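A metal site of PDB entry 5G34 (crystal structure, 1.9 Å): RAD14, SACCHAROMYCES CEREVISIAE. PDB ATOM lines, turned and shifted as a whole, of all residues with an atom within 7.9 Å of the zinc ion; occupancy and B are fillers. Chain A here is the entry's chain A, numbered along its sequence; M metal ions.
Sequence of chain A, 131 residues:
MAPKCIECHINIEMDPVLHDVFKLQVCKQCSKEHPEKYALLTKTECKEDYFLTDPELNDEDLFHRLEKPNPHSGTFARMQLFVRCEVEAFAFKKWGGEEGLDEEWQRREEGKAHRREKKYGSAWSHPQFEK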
ATOM      1  N   LYS A   4       5.952 -23.766  28.242  1.00  0.00           N
ATOM      2  CA  LYS A   4       5.841 -22.447  27.596  1.00  0.00           C
ATOM      3  C   LYS A   4       4.537 -21.743  27.917  1.00  0.00           C
ATOM      4  O   LYS A   4       3.505 -22.358  28.165  1.00  0.00           O
ATOM      5  CB  LYS A   4       5.886 -22.489  26.053  1.00  0.00           C
ATOM      6  CG  LYS A   4       6.870 -23.380  25.340  1.00  0.00           C
ATOM      7  CD  LYS A   4       8.279 -23.086  25.784  1.00  0.00           C
ATOM      8  CE  LYS A   4       9.180 -24.189  25.245  1.00  0.00           C
ATOM      9  NZ  LYS A   4       9.883 -23.664  24.059  1.00  0.00           N
ATOM     10  N   CYS A   5       4.571 -20.425  27.818  1.00  0.00           N
ATOM     11  CA  CYS A   5       3.413 -19.614  27.937  1.00  0.00           C
ATOM     12  C   CYS A   5       2.411 -20.074  26.855  1.00  0.00           C
ATOM     13  O   CYS A   5       2.733 -20.274  25.694  1.00  0.00           O
ATOM     14  CB  CYS A   5       3.767 -18.163  27.744  1.00  0.00           C
ATOM     15  SG  CYS A   5       2.412 -17.036  27.506  1.00  0.00           S
ATOM     16  N   ILE A   6       1.176 -20.235  27.288  1.00  0.00           N
ATOM     17  CA  ILE A   6       0.099 -20.671  26.441  1.00  0.00           C
ATOM     18  C   ILE A   6      -0.280 -19.623  25.464  1.00  0.00           C
ATOM     19  O   ILE A   6      -1.015 -19.937  24.523  1.00  0.00           O
ATOM     20  CB  ILE A   6      -1.144 -21.065  27.251  1.00  0.00           C
ATOM     21  CG1 ILE A   6      -1.778 -19.817  27.898  1.00  0.00           C
ATOM     22  CG2 ILE A   6      -0.773 -22.162  28.266  1.00  0.00           C
ATOM     23  CD1 ILE A   6      -2.600 -20.094  29.173  1.00  0.00           C
ATOM     24  N   GLU A   7       0.153 -18.371  25.598  1.00  0.00           N
ATOM     25  CA  GLU A   7      -0.238 -17.352  24.572  1.00  0.00           C
ATOM     26  C   GLU A   7       0.832 -17.185  23.549  1.00  0.00           C
ATOM     27  O   GLU A   7       0.542 -17.140  22.406  1.00  0.00           O
ATOM     28  CB  GLU A   7      -0.517 -15.980  25.185  1.00  0.00           C
ATOM     29  CG  GLU A   7      -1.747 -15.934  26.004  1.00  0.00           C
ATOM     30  CD  GLU A   7      -3.059 -15.948  25.252  1.00  0.00           C
ATOM     31  OE1 GLU A   7      -3.158 -15.589  24.093  1.00  0.00           O
ATOM     32  OE2 GLU A   7      -4.042 -16.302  25.859  1.00  0.00           O
ATOM     33  N   CYS A   8       2.091 -17.083  23.934  1.00  0.00           N
ATOM     34  CA  CYS A   8       3.134 -16.802  22.960  1.00  0.00           C
ATOM     35  C   CYS A   8       3.831 -18.069  22.522  1.00  0.00           C
ATOM     36  O   CYS A   8       4.480 -18.074  21.460  1.00  0.00           O
ATOM     37  CB  CYS A   8       4.150 -15.761  23.424  1.00  0.00           C
ATOM     38  SG  CYS A   8       5.048 -16.095  24.981  1.00  0.00           S
ATOM     39  N   HIS A   9       3.741 -19.128  23.315  1.00  0.00           N
ATOM     40  CA  HIS A   9       4.527 -20.349  23.117  1.00  0.00           C
ATOM     41  C   HIS A   9       6.014 -20.150  23.107  1.00  0.00           C
ATOM     42  O   HIS A   9       6.755 -21.011  22.555  1.00  0.00           O
ATOM     43  CB  HIS A   9       4.079 -21.144  21.861  1.00  0.00           C
ATOM     44  CG  HIS A   9       2.606 -21.107  21.675  1.00  0.00           C
ATOM     45  ND1 HIS A   9       1.739 -21.608  22.636  1.00  0.00           N
ATOM     46  CD2 HIS A   9       1.826 -20.545  20.705  1.00  0.00           C
ATOM     47  CE1 HIS A   9       0.485 -21.418  22.233  1.00  0.00           C
ATOM     48  NE2 HIS A   9       0.509 -20.788  21.061  1.00  0.00           N
ATOM     49  N   ILE A  10       6.493 -19.051  23.719  1.00  0.00           N
ATOM     50  CA  ILE A  10       7.943 -18.740  23.722  1.00  0.00           C
ATOM     51  C   ILE A  10       8.538 -18.632  25.084  1.00  0.00           C
ATOM     52  O   ILE A  10       9.535 -19.309  25.432  1.00  0.00           O
ATOM     53  CB  ILE A  10       8.193 -17.464  22.882  1.00  0.00           C
ATOM     54  CG1 ILE A  10       7.897 -17.815  21.390  1.00  0.00           C
ATOM     55  CG2 ILE A  10       9.629 -16.950  23.029  1.00  0.00           C
ATOM     56  CD1 ILE A  10       7.440 -16.651  20.523  1.00  0.00           C
ATOM     57  N   ASN A  11       7.945 -17.778  25.905  1.00  0.00           N
ATOM     58  CA  ASN A  11       8.468 -17.547  27.252  1.00  0.00           C
ATOM     59  C   ASN A  11       8.260 -18.734  28.129  1.00  0.00           C
ATOM     60  O   ASN A  11       7.345 -19.477  27.949  1.00  0.00           O
ATOM     61  CB  ASN A  11       7.907 -16.298  27.901  1.00  0.00           C
ATOM     62  CG  ASN A  11       8.662 -15.032  27.503  1.00  0.00           C
ATOM     63  OD1 ASN A  11       9.905 -15.050  27.308  1.00  0.00           O
ATOM     64  ND2 ASN A  11       7.920 -13.924  27.399  1.00  0.00           N
ATOM     65  N   ILE A  12       9.273 -18.989  28.954  1.00  0.00           N
ATOM     66  CA  ILE A  12       9.244 -19.996  29.974  1.00  0.00           C
ATOM     67  C   ILE A  12       9.038 -19.372  31.388  1.00  0.00           C
ATOM     68  O   ILE A  12       8.650 -20.114  32.283  1.00  0.00           O
ATOM     69  CB  ILE A  12      10.451 -20.995  29.864  1.00  0.00           C
ATOM     70  CG1 ILE A  12      11.803 -20.302  29.947  1.00  0.00           C
ATOM     71  CG2 ILE A  12      10.393 -21.775  28.572  1.00  0.00           C
ATOM     72  CD1 ILE A  12      12.966 -21.282  29.972  1.00  0.00           C
ATOM     73  N   GLU A  13       9.243 -18.060  31.622  1.00  0.00           N
ATOM     74  CA  GLU A  13       9.089 -17.439  32.943  1.00  0.00           C
ATOM     75  C   GLU A  13       7.682 -16.895  32.973  1.00  0.00           C
ATOM     76  O   GLU A  13       7.306 -16.064  32.101  1.00  0.00           O
ATOM     77  CB  GLU A  13       9.973 -16.232  33.163  1.00  0.00           C
ATOM     78  CG  GLU A  13      11.422 -16.542  33.218  1.00  0.00           C
ATOM     79  CD  GLU A  13      11.764 -17.421  34.389  1.00  0.00           C
ATOM     80  OE1 GLU A  13      11.262 -17.181  35.539  1.00  0.00           O
ATOM     81  OE2 GLU A  13      12.519 -18.389  34.096  1.00  0.00           O
ATOM     82  N   MET A  14       6.865 -17.427  33.851  1.00  0.00           N
ATOM     83  CA  MET A  14       5.457 -17.122  33.868  1.00  0.00           C
ATOM     84  C   MET A  14       5.243 -15.966  34.822  1.00  0.00           C
ATOM     85  O   MET A  14       6.041 -15.742  35.695  1.00  0.00           O
ATOM     86  CB  MET A  14       4.614 -18.303  34.350  1.00  0.00           C
ATOM     87  CG  MET A  14       4.783 -19.536  33.533  1.00  0.00           C
ATOM     88  SD  MET A  14       4.422 -19.274  31.766  1.00  0.00           S
ATOM     89  CE  MET A  14       5.542 -20.570  31.230  1.00  0.00           C
ATOM     90  N   GLN A  25      -0.634 -20.447  33.050  1.00  0.00           N
ATOM     91  CA  GLN A  25       0.726 -20.548  32.545  1.00  0.00           C
ATOM     92  C   GLN A  25       0.892 -19.448  31.460  1.00  0.00           C
ATOM     93  O   GLN A  25       0.963 -19.786  30.239  1.00  0.00           O
ATOM     94  CB  GLN A  25       0.951 -21.894  31.857  1.00  0.00           C
ATOM     95  CG  GLN A  25       0.712 -23.032  32.751  1.00  0.00           C
ATOM     96  CD  GLN A  25       1.991 -23.677  33.164  1.00  0.00           C
ATOM     97  OE1 GLN A  25       2.599 -24.486  32.377  1.00  0.00           O
ATOM     98  NE2 GLN A  25       2.403 -23.389  34.405  1.00  0.00           N
ATOM     99  N   VAL A  26       0.935 -18.187  31.925  1.00  0.00           N
ATOM    100  CA  VAL A  26       0.991 -17.013  31.067  1.00  0.00           C
ATOM    101  C   VAL A  26       2.079 -16.050  31.496  1.00  0.00           C
ATOM    102  O   VAL A  26       2.228 -15.828  32.725  1.00  0.00           O
ATOM    103  CB  VAL A  26      -0.342 -16.259  31.089  1.00  0.00           C
ATOM    104  CG1 VAL A  26      -0.318 -15.180  30.063  1.00  0.00           C
ATOM    105  CG2 VAL A  26      -1.512 -17.200  30.746  1.00  0.00           C
ATOM    106  N   CYS A  27       2.845 -15.516  30.509  1.00  0.00           N
ATOM    107  CA  CYS A  27       3.970 -14.690  30.800  1.00  0.00           C
ATOM    108  C   CYS A  27       3.410 -13.327  31.070  1.00  0.00           C
ATOM    109  O   CYS A  27       2.353 -12.985  30.590  1.00  0.00           O
ATOM    110  CB  CYS A  27       5.109 -14.676  29.712  1.00  0.00           C
ATOM    111  SG  CYS A  27       4.657 -13.896  28.158  1.00  0.00           S
ATOM    112  N   LYS A  28       4.142 -12.541  31.788  1.00  0.00           N
ATOM    113  CA  LYS A  28       3.756 -11.166  32.036  1.00  0.00           C
ATOM    114  C   LYS A  28       3.465 -10.348  30.760  1.00  0.00           C
ATOM    115  O   LYS A  28       2.404  -9.686  30.655  1.00  0.00           O
ATOM    116  CB  LYS A  28       4.870 -10.554  32.842  1.00  0.00           C
ATOM    117  CG  LYS A  28       4.750  -9.104  33.122  1.00  0.00           C
ATOM    118  CD  LYS A  28       3.629  -8.844  34.057  1.00  0.00           C
ATOM    119  CE  LYS A  28       3.921  -7.625  34.986  1.00  0.00           C
ATOM    120  NZ  LYS A  28       3.304  -7.962  36.334  1.00  0.00           N
ATOM    121  N   GLN A  29       4.357 -10.427  29.789  1.00  0.00           N
ATOM    122  CA  GLN A  29       4.160  -9.703  28.548  1.00  0.00           C
ATOM    123  C   GLN A  29       2.789 -10.053  27.868  1.00  0.00           C
ATOM    124  O   GLN A  29       2.039  -9.191  27.505  1.00  0.00           O
ATOM    125  CB  GLN A  29       5.351  -9.950  27.622  1.00  0.00           C
ATOM    126  CG  GLN A  29       5.217  -9.229  26.315  1.00  0.00           C
ATOM    127  CD  GLN A  29       6.550  -9.168  25.503  1.00  0.00           C
ATOM    128  OE1 GLN A  29       7.552  -9.686  25.849  1.00  0.00           O
ATOM    129  NE2 GLN A  29       6.447  -8.563  24.374  1.00  0.00           N
ATOM    130  N   CYS A  30       2.483 -11.335  27.745  1.00  0.00           N
ATOM    131  CA  CYS A  30       1.225 -11.757  27.132  1.00  0.00           C
ATOM    132  C   CYS A  30       0.010 -11.292  27.957  1.00  0.00           C
ATOM    133  O   CYS A  30      -1.002 -10.899  27.418  1.00  0.00           O
ATOM    134  CB  CYS A  30       1.227 -13.276  26.949  1.00  0.00           C
ATOM    135  SG  CYS A  30       2.331 -13.779  25.649  1.00  0.00           S
ATOM    136  N   SER A  31       0.174 -11.196  29.250  1.00  0.00           N
ATOM    137  CA  SER A  31      -0.873 -10.701  30.101  1.00  0.00           C
ATOM    138  C   SER A  31      -1.213  -9.211  29.827  1.00  0.00           C
ATOM    139  O   SER A  31      -2.397  -8.814  29.867  1.00  0.00           O
ATOM    140  CB  SER A  31      -0.527 -10.945  31.574  1.00  0.00           C
ATOM    141  OG  SER A  31       0.207  -9.899  32.162  1.00  0.00           O
ATOM    142  N   GLU A  33      -0.548  -7.837  26.881  1.00  0.00           N
ATOM    143  CA  GLU A  33      -1.079  -7.859  25.521  1.00  0.00           C
ATOM    144  C   GLU A  33      -2.489  -8.367  25.392  1.00  0.00           C
ATOM    145  O   GLU A  33      -3.154  -8.057  24.377  1.00  0.00           O
ATOM    146  CB  GLU A  33      -0.141  -8.685  24.666  1.00  0.00           C
ATOM    147  CG  GLU A  33       1.164  -7.927  24.405  1.00  0.00           C
ATOM    148  CD  GLU A  33       2.338  -8.754  23.870  1.00  0.00           C
ATOM    149  OE1 GLU A  33       2.295  -9.993  23.835  1.00  0.00           O
ATOM    150  OE2 GLU A  33       3.342  -8.118  23.503  1.00  0.00           O
ATOM    151  N   HIS A  34      -3.016  -9.080  26.418  1.00  0.00           N
ATOM    152  CA  HIS A  34      -4.395  -9.508  26.361  1.00  0.00           C
ATOM    153  C   HIS A  34      -5.191  -9.251  27.637  1.00  0.00           C
ATOM    154  O   HIS A  34      -5.520 -10.182  28.341  1.00  0.00           O
ATOM    155  CB  HIS A  34      -4.424 -11.004  26.067  1.00  0.00           C
ATOM    156  CG  HIS A  34      -3.746 -11.382  24.806  1.00  0.00           C
ATOM    157  ND1 HIS A  34      -4.262 -11.066  23.583  1.00  0.00           N
ATOM    158  CD2 HIS A  34      -2.548 -11.955  24.579  1.00  0.00           C
ATOM    159  CE1 HIS A  34      -3.445 -11.507  22.642  1.00  0.00           C
ATOM    160  NE2 HIS A  34      -2.399 -12.063  23.232  1.00  0.00           N
HETATM  161 ZN    ZN M   1       3.674 -15.280  26.630  1.00  0.00          ZN
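The zinc ion is bound by SG of Cys 30 (2.2 Å). The zinc ion is bound by the side-chain sulfur (SG) of Cys 27, 2.3 Å away. The zinc ion is bound by SG of Cys 8 (2.3 Å). The zinc ion is bound by SG of Cys 5 (2.3 Å).
The backbone NH (N) of Cys 5 lies within hydrogen-bond range of the backbone carbonyl oxygen (O) of Asn 11. SG of Cys 8 sits close to N of Asn 11 (3.5 Å). O of Cys 5 lies close to ND1 of His 9 (3.5 Å). The side-chain amide nitrogen (ND2) of Asn 11 sits close to the side-chain sulfur (SG) of Cys 27 (3.4 Å). The backbone NH of Glu 7 sits close to the side-chain sulfur of Cys 5 (3.2 Å). The side-chain sulfur of Cys 8 sits close to the backbone NH of Ile 10 (3.5 Å).
Four residues have an atom within 4 Å of the zinc ion: Cys 5, Cys 8, Cys 27 and Cys 30.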
